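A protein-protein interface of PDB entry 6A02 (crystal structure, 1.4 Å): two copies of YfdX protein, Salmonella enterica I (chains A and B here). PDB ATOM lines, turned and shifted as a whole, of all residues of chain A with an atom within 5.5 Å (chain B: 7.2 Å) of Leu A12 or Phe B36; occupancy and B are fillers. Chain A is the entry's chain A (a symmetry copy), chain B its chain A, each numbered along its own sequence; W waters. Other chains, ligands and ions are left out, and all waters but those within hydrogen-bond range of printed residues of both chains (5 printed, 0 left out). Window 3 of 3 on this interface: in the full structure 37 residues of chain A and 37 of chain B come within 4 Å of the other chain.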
ATOM      1  N   VAL A  10       0.156   4.887   4.020  1.00  0.00           N
ATOM      2  CA  VAL A  10       1.441   5.571   3.908  1.00  0.00           C
ATOM      3  C   VAL A  10       1.456   6.818   4.779  1.00  0.00           C
ATOM      4  O   VAL A  10       0.413   7.419   5.064  1.00  0.00           O
ATOM      5  CB  VAL A  10       1.803   5.947   2.450  1.00  0.00           C
ATOM      6  CG1 VAL A  10       1.911   4.704   1.583  1.00  0.00           C
ATOM      7  CG2 VAL A  10       0.778   6.910   1.869  1.00  0.00           C
ATOM      8  N   THR A  11       2.657   7.217   5.179  1.00  0.00           N
ATOM      9  CA  THR A  11       2.856   8.454   5.919  1.00  0.00           C
ATOM     10  C   THR A  11       2.738   9.660   4.982  1.00  0.00           C
ATOM     11  O   THR A  11       2.560   9.530   3.765  1.00  0.00           O
ATOM     12  CB  THR A  11       4.240   8.465   6.565  1.00  0.00           C
ATOM     13  OG1 THR A  11       5.237   8.550   5.537  1.00  0.00           O
ATOM     14  CG2 THR A  11       4.464   7.201   7.401  1.00  0.00           C
ATOM     15  N   LEU A  12       2.865  10.861   5.559  1.00  0.00           N
ATOM     16  CA  LEU A  12       2.823  12.073   4.746  1.00  0.00           C
ATOM     17  C   LEU A  12       3.933  12.091   3.705  1.00  0.00           C
ATOM     18  O   LEU A  12       3.753  12.659   2.621  1.00  0.00           O
ATOM     19  CB  LEU A  12       2.899  13.322   5.625  1.00  0.00           C
ATOM     20  CG  LEU A  12       1.723  13.549   6.578  1.00  0.00           C
ATOM     21  CD1 LEU A  12       1.984  14.747   7.487  1.00  0.00           C
ATOM     22  CD2 LEU A  12       0.419  13.726   5.800  1.00  0.00           C
ATOM     23  N   ASN A  13       5.075  11.474   4.013  1.00  0.00           N
ATOM     24  CA  ASN A  13       6.200  11.374   3.092  1.00  0.00           C
ATOM     25  C   ASN A  13       6.137  10.130   2.215  1.00  0.00           C
ATOM     26  O   ASN A  13       7.136   9.802   1.565  1.00  0.00           O
ATOM     27  CB  ASN A  13       7.524  11.375   3.861  1.00  0.00           C
ATOM     28  CG  ASN A  13       8.036  12.761   4.135  1.00  0.00           C
ATOM     29  OD1 ASN A  13       7.806  13.312   5.212  1.00  0.00           O
ATOM     30  ND2 ASN A  13       8.738  13.340   3.162  1.00  0.00           N
ATOM     31  N   ASN A  14       5.001   9.430   2.198  1.00  0.00           N
ATOM     32  CA  ASN A  14       4.745   8.287   1.320  1.00  0.00           C
ATOM     33  C   ASN A  14       5.507   7.030   1.718  1.00  0.00           C
ATOM     34  O   ASN A  14       5.726   6.151   0.880  1.00  0.00           O
ATOM     35  CB  ASN A  14       4.956   8.610  -0.169  1.00  0.00           C
ATOM     36  CG  ASN A  14       4.104   9.776  -0.642  1.00  0.00           C
ATOM     37  OD1 ASN A  14       2.927   9.886  -0.292  1.00  0.00           O
ATOM     38  ND2 ASN A  14       4.703  10.664  -1.435  1.00  0.00           N
ATOM     39  N   SER A  83       0.059   6.232  11.696  1.00  0.00           N
ATOM     40  CA  SER A  83       0.359   7.654  11.671  1.00  0.00           C
ATOM     41  C   SER A  83      -0.873   8.443  12.080  1.00  0.00           C
ATOM     42  O   SER A  83      -1.999   8.116  11.683  1.00  0.00           O
ATOM     43  CB  SER A  83       0.768   8.135  10.284  1.00  0.00           C
ATOM     44  OG  SER A  83       1.623   9.254  10.416  1.00  0.00           O
ATOM     45  N   ILE A  85      -2.095  12.824  13.260  1.00  0.00           N
ATOM     46  CA  ILE A  85      -1.774  14.240  13.132  1.00  0.00           C
ATOM     47  C   ILE A  85      -2.042  14.950  14.454  1.00  0.00           C
ATOM     48  O   ILE A  85      -3.058  14.696  15.109  1.00  0.00           O
ATOM     49  CB  ILE A  85      -2.624  14.878  12.013  1.00  0.00           C
ATOM     50  CG1 ILE A  85      -2.305  14.219  10.669  1.00  0.00           C
ATOM     51  CG2 ILE A  85      -2.406  16.388  11.937  1.00  0.00           C
ATOM     52  CD1 ILE A  85      -0.905  14.480  10.195  1.00  0.00           C
ATOM     53  N   VAL A  87      -2.353  19.058  15.395  1.00  0.00           N
ATOM     54  CA  VAL A  87      -2.344  20.447  14.953  1.00  0.00           C
ATOM     55  C   VAL A  87      -2.125  21.349  16.161  1.00  0.00           C
ATOM     56  O   VAL A  87      -2.480  21.008  17.296  1.00  0.00           O
ATOM     57  CB  VAL A  87      -3.636  20.832  14.200  1.00  0.00           C
ATOM     58  CG1 VAL A  87      -3.757  20.023  12.927  1.00  0.00           C
ATOM     59  CG2 VAL A  87      -4.853  20.614  15.094  1.00  0.00           C
ATOM     60  N   MET A 108      -6.242  20.336   0.258  1.00  0.00           N
ATOM     61  CA  MET A 108      -6.572  18.954   0.604  1.00  0.00           C
ATOM     62  C   MET A 108      -7.420  18.302  -0.478  1.00  0.00           C
ATOM     63  O   MET A 108      -7.159  17.161  -0.878  1.00  0.00           O
ATOM     64  CB  MET A 108      -7.275  18.890   1.960  1.00  0.00           C
ATOM     65  CG  MET A 108      -6.312  19.007   3.116  1.00  0.00           C
ATOM     66  SD  MET A 108      -7.097  18.880   4.733  1.00  0.00           S
ATOM     67  CE  MET A 108      -7.678  20.557   4.916  1.00  0.00           C
ATOM     68  N   LYS A 113      -0.272  17.802  -0.590  1.00  0.00           N
ATOM     69  CA  LYS A 113       0.126  17.763   0.816  1.00  0.00           C
ATOM     70  C   LYS A 113       0.958  18.982   1.185  1.00  0.00           C
ATOM     71  O   LYS A 113       0.703  19.636   2.201  1.00  0.00           O
ATOM     72  CB  LYS A 113       0.913  16.488   1.123  1.00  0.00           C
ATOM     73  CG  LYS A 113       0.176  15.195   0.876  1.00  0.00           C
ATOM     74  CD  LYS A 113       0.976  14.029   1.440  1.00  0.00           C
ATOM     75  CE  LYS A 113       0.742  12.742   0.662  1.00  0.00           C
ATOM     76  NZ  LYS A 113       1.385  11.555   1.319  1.00  0.00           N
ATOM     77  N   THR A 116      -1.093  21.990   1.383  1.00  0.00           N
ATOM     78  CA  THR A 116      -1.919  21.958   2.587  1.00  0.00           C
ATOM     79  C   THR A 116      -1.136  22.463   3.791  1.00  0.00           C
ATOM     80  O   THR A 116      -1.612  23.329   4.538  1.00  0.00           O
ATOM     81  CB  THR A 116      -2.423  20.533   2.828  1.00  0.00           C
ATOM     82  OG1 THR A 116      -3.239  20.131   1.721  1.00  0.00           O
ATOM     83  CG2 THR A 116      -3.244  20.461   4.111  1.00  0.00           C
ATOM     84  N   ILE A 117       0.077  21.941   3.983  1.00  0.00           N
ATOM     85  CA  ILE A 117       0.921  22.386   5.091  1.00  0.00           C
ATOM     86  C   ILE A 117       1.169  23.884   5.005  1.00  0.00           C
ATOM     87  O   ILE A 117       1.085  24.605   6.009  1.00  0.00           O
ATOM     88  CB  ILE A 117       2.232  21.579   5.123  1.00  0.00           C
ATOM     89  CG1 ILE A 117       1.932  20.081   5.240  1.00  0.00           C
ATOM     90  CG2 ILE A 117       3.130  22.054   6.255  1.00  0.00           C
ATOM     91  CD1 ILE A 117       1.031  19.729   6.413  1.00  0.00           C
ATOM     92  N   LEU A 120      -2.010  25.861   5.796  1.00  0.00           N
ATOM     93  CA  LEU A 120      -2.302  25.806   7.224  1.00  0.00           C
ATOM     94  C   LEU A 120      -1.395  26.739   8.014  1.00  0.00           C
ATOM     95  O   LEU A 120      -1.832  27.352   8.998  1.00  0.00           O
ATOM     96  CB  LEU A 120      -2.219  24.365   7.733  1.00  0.00           C
ATOM     97  CG  LEU A 120      -3.407  23.500   7.296  1.00  0.00           C
ATOM     98  CD1 LEU A 120      -3.190  22.050   7.698  1.00  0.00           C
ATOM     99  CD2 LEU A 120      -4.708  24.024   7.881  1.00  0.00           C
ATOM    100  N   VAL A 127       1.605  21.601  11.884  1.00  0.00           N
ATOM    101  CA  VAL A 127       1.223  20.198  11.746  1.00  0.00           C
ATOM    102  C   VAL A 127       2.387  19.331  12.202  1.00  0.00           C
ATOM    103  O   VAL A 127       3.527  19.525  11.761  1.00  0.00           O
ATOM    104  CB  VAL A 127       0.828  19.844  10.299  1.00  0.00           C
ATOM    105  CG1 VAL A 127       0.498  18.364  10.186  1.00  0.00           C
ATOM    106  CG2 VAL A 127      -0.374  20.667   9.873  1.00  0.00           C
ATOM    107  N   GLU A 129       3.338  15.129  12.621  1.00  0.00           N
ATOM    108  CA  GLU A 129       2.933  13.767  12.318  1.00  0.00           C
ATOM    109  C   GLU A 129       3.475  12.837  13.399  1.00  0.00           C
ATOM    110  O   GLU A 129       4.681  12.844  13.682  1.00  0.00           O
ATOM    111  CB  GLU A 129       3.443  13.338  10.944  1.00  0.00           C
ATOM    112  CG  GLU A 129       2.990  11.962  10.573  1.00  0.00           C
ATOM    113  CD  GLU A 129       3.559  11.468   9.265  1.00  0.00           C
ATOM    114  OE1 GLU A 129       4.722  11.797   8.945  1.00  0.00           O
ATOM    115  OE2 GLU A 129       2.840  10.726   8.570  1.00  0.00           O
ATOM    116  N   VAL A 176       6.456  18.332   9.846  1.00  0.00           N
ATOM    117  CA  VAL A 176       6.258  17.853   8.485  1.00  0.00           C
ATOM    118  C   VAL A 176       7.256  18.549   7.571  1.00  0.00           C
ATOM    119  O   VAL A 176       7.241  19.778   7.441  1.00  0.00           O
ATOM    120  CB  VAL A 176       4.814  18.092   8.025  1.00  0.00           C
ATOM    121  CG1 VAL A 176       4.592  17.487   6.650  1.00  0.00           C
ATOM    122  CG2 VAL A 176       3.848  17.510   9.035  1.00  0.00           C
ATOM    123  N   LEU A 178       8.179  17.839   3.828  1.00  0.00           N
ATOM    124  CA  LEU A 178       7.912  17.072   2.617  1.00  0.00           C
ATOM    125  C   LEU A 178       8.950  17.343   1.531  1.00  0.00           C
ATOM    126  O   LEU A 178       9.802  16.494   1.254  1.00  0.00           O
ATOM    127  CB  LEU A 178       6.508  17.383   2.107  1.00  0.00           C
ATOM    128  CG  LEU A 178       5.415  17.085   3.130  1.00  0.00           C
ATOM    129  CD1 LEU A 178       4.050  17.411   2.567  1.00  0.00           C
ATOM    130  CD2 LEU A 178       5.486  15.626   3.580  1.00  0.00           C
ATOM    131  N   SER B  31      -9.508   8.201   9.116  1.00  0.00           N
ATOM    132  CA  SER B  31     -10.167   9.199   8.283  1.00  0.00           C
ATOM    133  C   SER B  31      -9.538  10.566   8.486  1.00  0.00           C
ATOM    134  O   SER B  31      -9.219  11.270   7.518  1.00  0.00           O
ATOM    135  CB  SER B  31     -11.658   9.234   8.615  1.00  0.00           C
ATOM    136  OG  SER B  31     -12.337  10.247   7.884  1.00  0.00           O
ATOM    137  N   ARG B  32      -9.339  10.967   9.745  1.00  0.00           N
ATOM    138  CA  ARG B  32      -8.756  12.281   9.998  1.00  0.00           C
ATOM    139  C   ARG B  32      -7.368  12.388   9.387  1.00  0.00           C
ATOM    140  O   ARG B  32      -7.026  13.404   8.774  1.00  0.00           O
ATOM    141  CB  ARG B  32      -8.704  12.568  11.498  1.00  0.00           C
ATOM    142  CG  ARG B  32      -8.073  13.907  11.818  1.00  0.00           C
ATOM    143  CD  ARG B  32      -8.342  14.296  13.264  1.00  0.00           C
ATOM    144  NE  ARG B  32      -7.701  15.551  13.631  1.00  0.00           N
ATOM    145  CZ  ARG B  32      -6.475  15.628  14.138  1.00  0.00           C
ATOM    146  NH1 ARG B  32      -5.765  14.525  14.322  1.00  0.00           N
ATOM    147  NH2 ARG B  32      -5.960  16.804  14.450  1.00  0.00           N
ATOM    148  N   PHE B  33      -6.550  11.346   9.542  1.00  0.00           N
ATOM    149  CA  PHE B  33      -5.213  11.396   8.968  1.00  0.00           C
ATOM    150  C   PHE B  33      -5.272  11.585   7.459  1.00  0.00           C
ATOM    151  O   PHE B  33      -4.493  12.367   6.889  1.00  0.00           O
ATOM    152  CB  PHE B  33      -4.438  10.122   9.297  1.00  0.00           C
ATOM    153  CG  PHE B  33      -3.089  10.067   8.626  1.00  0.00           C
ATOM    154  CD1 PHE B  33      -2.025  10.799   9.123  1.00  0.00           C
ATOM    155  CD2 PHE B  33      -2.911   9.339   7.464  1.00  0.00           C
ATOM    156  CE1 PHE B  33      -0.777  10.776   8.482  1.00  0.00           C
ATOM    157  CE2 PHE B  33      -1.668   9.313   6.827  1.00  0.00           C
ATOM    158  CZ  PHE B  33      -0.609  10.033   7.339  1.00  0.00           C
ATOM    159  N   GLU B  34      -6.189  10.877   6.793  1.00  0.00           N
ATOM    160  CA  GLU B  34      -6.239  10.947   5.335  1.00  0.00           C
ATOM    161  C   GLU B  34      -6.637  12.334   4.830  1.00  0.00           C
ATOM    162  O   GLU B  34      -6.281  12.696   3.705  1.00  0.00           O
ATOM    163  CB  GLU B  34      -7.124   9.839   4.770  1.00  0.00           C
ATOM    164  CG  GLU B  34      -6.606   8.431   5.036  1.00  0.00           C
ATOM    165  CD  GLU B  34      -5.271   8.128   4.376  1.00  0.00           C
ATOM    166  OE1 GLU B  34      -4.750   8.969   3.612  1.00  0.00           O
ATOM    167  OE2 GLU B  34      -4.736   7.025   4.626  1.00  0.00           O
ATOM    168  N   LEU B  35      -7.362  13.123   5.631  1.00  0.00           N
ATOM    169  CA  LEU B  35      -7.629  14.509   5.246  1.00  0.00           C
ATOM    170  C   LEU B  35      -6.330  15.282   5.059  1.00  0.00           C
ATOM    171  O   LEU B  35      -6.129  15.953   4.037  1.00  0.00           O
ATOM    172  CB  LEU B  35      -8.501  15.195   6.296  1.00  0.00           C
ATOM    173  CG  LEU B  35      -9.909  14.642   6.486  1.00  0.00           C
ATOM    174  CD1 LEU B  35     -10.579  15.285   7.694  1.00  0.00           C
ATOM    175  CD2 LEU B  35     -10.740  14.841   5.219  1.00  0.00           C
ATOM    176  N   PHE B  36      -5.431  15.195   6.043  1.00  0.00           N
ATOM    177  CA  PHE B  36      -4.146  15.880   5.958  1.00  0.00           C
ATOM    178  C   PHE B  36      -3.222  15.236   4.937  1.00  0.00           C
ATOM    179  O   PHE B  36      -2.301  15.893   4.440  1.00  0.00           O
ATOM    180  CB  PHE B  36      -3.482  15.901   7.337  1.00  0.00           C
ATOM    181  CG  PHE B  36      -4.227  16.726   8.345  1.00  0.00           C
ATOM    182  CD1 PHE B  36      -3.947  18.076   8.479  1.00  0.00           C
ATOM    183  CD2 PHE B  36      -5.214  16.164   9.146  1.00  0.00           C
ATOM    184  CE1 PHE B  36      -4.636  18.853   9.399  1.00  0.00           C
ATOM    185  CE2 PHE B  36      -5.903  16.937  10.079  1.00  0.00           C
ATOM    186  CZ  PHE B  36      -5.611  18.286  10.200  1.00  0.00           C
ATOM    187  N   ASN B  37      -3.436  13.963   4.630  1.00  0.00           N
ATOM    188  CA  ASN B  37      -2.619  13.209   3.689  1.00  0.00           C
ATOM    189  C   ASN B  37      -3.045  13.436   2.239  1.00  0.00           C
ATOM    190  O   ASN B  37      -2.564  12.725   1.347  1.00  0.00           O
ATOM    191  CB  ASN B  37      -2.698  11.720   4.053  1.00  0.00           C
ATOM    192  CG  ASN B  37      -1.534  10.912   3.510  1.00  0.00           C
ATOM    193  OD1 ASN B  37      -0.433  11.429   3.320  1.00  0.00           O
ATOM    194  ND2 ASN B  37      -1.774   9.621   3.269  1.00  0.00           N
ATOM    195  N   GLY B  38      -3.943  14.389   1.996  1.00  0.00           N
ATOM    196  CA  GLY B  38      -4.378  14.671   0.640  1.00  0.00           C
ATOM    197  C   GLY B  38      -5.212  13.583   0.007  1.00  0.00           C
ATOM    198  O   GLY B  38      -5.254  13.484  -1.224  1.00  0.00           O
ATOM    199  N   ARG B  39      -5.887  12.765   0.803  1.00  0.00           N
ATOM    200  CA  ARG B  39      -6.722  11.680   0.305  1.00  0.00           C
ATOM    201  C   ARG B  39      -8.123  11.854   0.883  1.00  0.00           C
ATOM    202  O   ARG B  39      -8.595  11.013   1.653  1.00  0.00           O
ATOM    203  CB  ARG B  39      -6.115  10.312   0.676  1.00  0.00           C
ATOM    204  CG  ARG B  39      -4.815   9.978  -0.058  1.00  0.00           C
ATOM    205  CD  ARG B  39      -4.160   8.732   0.526  1.00  0.00           C
ATOM    206  NE  ARG B  39      -3.246   8.071  -0.409  1.00  0.00           N
ATOM    207  CZ  ARG B  39      -1.970   8.406  -0.590  1.00  0.00           C
ATOM    208  NH1 ARG B  39      -1.434   9.418   0.083  1.00  0.00           N
ATOM    209  NH2 ARG B  39      -1.227   7.738  -1.465  1.00  0.00           N
ATOM    210  N   THR B  40      -8.791  12.951   0.507  1.00  0.00           N
ATOM    211  CA  THR B  40     -10.088  13.253   1.113  1.00  0.00           C
ATOM    212  C   THR B  40     -11.150  12.226   0.741  1.00  0.00           C
ATOM    213  O   THR B  40     -12.068  11.977   1.528  1.00  0.00           O
ATOM    214  CB  THR B  40     -10.569  14.666   0.759  1.00  0.00           C
ATOM    215  OG1 THR B  40     -10.727  14.768  -0.664  1.00  0.00           O
ATOM    216  CG2 THR B  40      -9.604  15.732   1.275  1.00  0.00           C
ATOM    217  N   ALA B  43     -10.713   9.514   3.095  1.00  0.00           N
ATOM    218  CA  ALA B  43     -11.246   9.924   4.389  1.00  0.00           C
ATOM    219  C   ALA B  43     -12.759   9.764   4.439  1.00  0.00           C
ATOM    220  O   ALA B  43     -13.315   9.319   5.448  1.00  0.00           O
ATOM    221  CB  ALA B  43     -10.863  11.368   4.682  1.00  0.00           C
ATOM    222  N   TYR B 155     -12.999  20.404   4.882  1.00  0.00           N
ATOM    223  CA  TYR B 155     -12.232  19.255   5.353  1.00  0.00           C
ATOM    224  C   TYR B 155     -11.591  19.515   6.707  1.00  0.00           C
ATOM    225  O   TYR B 155     -11.637  18.646   7.584  1.00  0.00           O
ATOM    226  CB  TYR B 155     -11.189  18.853   4.315  1.00  0.00           C
ATOM    227  CG  TYR B 155     -11.801  18.499   2.985  1.00  0.00           C
ATOM    228  CD1 TYR B 155     -12.620  17.389   2.853  1.00  0.00           C
ATOM    229  CD2 TYR B 155     -11.575  19.288   1.864  1.00  0.00           C
ATOM    230  CE1 TYR B 155     -13.186  17.063   1.624  1.00  0.00           C
ATOM    231  CE2 TYR B 155     -12.138  18.975   0.646  1.00  0.00           C
ATOM    232  CZ  TYR B 155     -12.942  17.864   0.538  1.00  0.00           C
ATOM    233  OH  TYR B 155     -13.514  17.534  -0.678  1.00  0.00           O
ATOM    234  N   TYR B 156     -10.978  20.685   6.896  1.00  0.00           N
ATOM    235  CA  TYR B 156     -10.380  20.986   8.194  1.00  0.00           C
ATOM    236  C   TYR B 156     -11.421  20.920   9.304  1.00  0.00           C
ATOM    237  O   TYR B 156     -11.166  20.369  10.388  1.00  0.00           O
ATOM    238  CB  TYR B 156      -9.731  22.370   8.175  1.00  0.00           C
ATOM    239  CG  TYR B 156      -8.864  22.592   9.390  1.00  0.00           C
ATOM    240  CD1 TYR B 156      -7.578  22.069   9.444  1.00  0.00           C
ATOM    241  CD2 TYR B 156      -9.329  23.313  10.483  1.00  0.00           C
ATOM    242  CE1 TYR B 156      -6.772  22.253  10.561  1.00  0.00           C
ATOM    243  CE2 TYR B 156      -8.529  23.499  11.609  1.00  0.00           C
ATOM    244  CZ  TYR B 156      -7.258  22.965  11.634  1.00  0.00           C
ATOM    245  OH  TYR B 156      -6.447  23.144  12.734  1.00  0.00           O
ATOM    246  N   GLY B 159     -12.145  17.457  10.172  1.00  0.00           N
ATOM    247  CA  GLY B 159     -11.078  16.911  10.993  1.00  0.00           C
ATOM    248  C   GLY B 159     -11.223  17.281  12.452  1.00  0.00           C
ATOM    249  O   GLY B 159     -10.946  16.465  13.340  1.00  0.00           O
ATOM    250  N   LEU B 160     -11.669  18.508  12.725  1.00  0.00           N
ATOM    251  CA  LEU B 160     -11.909  18.923  14.105  1.00  0.00           C
ATOM    252  C   LEU B 160     -12.963  18.053  14.776  1.00  0.00           C
ATOM    253  O   LEU B 160     -12.824  17.690  15.954  1.00  0.00           O
ATOM    254  CB  LEU B 160     -12.352  20.380  14.134  1.00  0.00           C
ATOM    255  CG  LEU B 160     -11.354  21.451  13.730  1.00  0.00           C
ATOM    256  CD1 LEU B 160     -12.069  22.799  13.725  1.00  0.00           C
ATOM    257  CD2 LEU B 160     -10.155  21.488  14.671  1.00  0.00           C
HETATM  258  O   HOH W   1      -7.911  14.758  -1.726  1.00  0.00           O
HETATM  259  O   HOH W   2      -3.067  17.267   1.782  1.00  0.00           O
HETATM  260  O   HOH W   3      -2.717   6.200   2.569  1.00  0.00           O
HETATM  261  O   HOH W   4      -2.298   6.376   5.160  1.00  0.00           O
HETATM  262  O   HOH W   5      -4.642  17.769  17.042  1.00  0.00           O
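NH1 of Arg B32 is in hydrogen-bond range of O of Ile A85, 2.8 Å away.
O of Leu B35 sits close to SD of Met A108, at 3.2 Å.
OD1 of Asn B37 lies within hydrogen-bond range of NZ of Lys A113 (2.7 Å).
The backbone carbonyl oxygen (O) of Leu A12 sits at hydrogen-bond distance from the side-chain amino group (NZ) of Lys A113 (2.9 Å).
OG of Ser A83 sits at hydrogen-bond distance from OE2 of Glu A129 (2.7 Å).
N of Arg B39 sits at hydrogen-bond distance from O of Glu B34.
N of Asn A14 lies within hydrogen-bond range of OG1 of Thr A11 (3.5 Å).
N of Asn A13 lies close to OG1 of Thr A11.
The backbone carbonyl oxygen (O) of Thr A11 sits at hydrogen-bond distance from the side-chain amino group (NZ) of Lys A113 (3.4 Å).
CE2 of Phe B33 touches O of Val A10, 3.3 Å away.
O of Val A10 touches ND2 of Asn B37, at 3.6 Å.
NH1 of Arg B39 touches CG2 of Val A10, 3.8 Å away.
Thr A11 touches Asn B37 (O to OD1, 3.6 Å).
Leu A12 touches Phe B33.
Leu A12 touches Phe B36.
Leu A12 touches Asn B37.
Phe B33 touches Ser A83 (CE1 to OG, 3.4 Å).
CG2 of Val A87 touches OH of Tyr B156, 3.8 Å away.
Lys A113 touches Arg B39.
Printed residues of chain B within 4 Å of Leu A12: Phe B33 (3.99 Å), Phe B36 (3.7 Å) and Asn B37 (3.5 Å).
Of chain A, only Leu A12, Ile A85, Val A87 and Leu A120 come within 4 Å of Phe B36.
Of the printed residues of chain A, Phe B33 touches Val A10, Leu A12, Ser A83, Ile A85 and Glu A129.
Printed residues of chain A within 4 Å of Tyr B155: Met A108.
Of the printed residues of chain B, Met A108 touches Leu B35, Thr B40, Tyr B155 and Tyr B156.
Of the 17 printed residues of chain A, 10 touch a printed residue of chain B.
Hydrophobic or aromatic side chains of chain A that line the printed part of chain B: Val A10, Leu A12, Ile A85, Val A87, Met A108 and Leu A120.
Along chain B the printed residues that touch a printed residue of chain A span positions 32 to 156.
Among the printed residues, 22 pairs touch across the chains.
No position is printed for both chains.
Water W4 bridges OE2 of Glu B34 (2.6 Å) and O of Val A10 (2.9 Å).
Water W1 lies within hydrogen-bond range of O of Met A108, O of Gly B38 and N of Thr B40.
Water W2 lies within hydrogen-bond range of OG1 of Thr A116 (2.9 Å), N of Gly B38 (3.0 Å) and O of Phe B36 (3.1 Å).
Water W3 bridges the side-chain carboxylate (OE2) of Glu B34 and the backbone NH (N) of Val A10.
Water W5 lies within hydrogen-bond range of the guanidinium group of Arg B32 and the backbone NH of Val A87.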
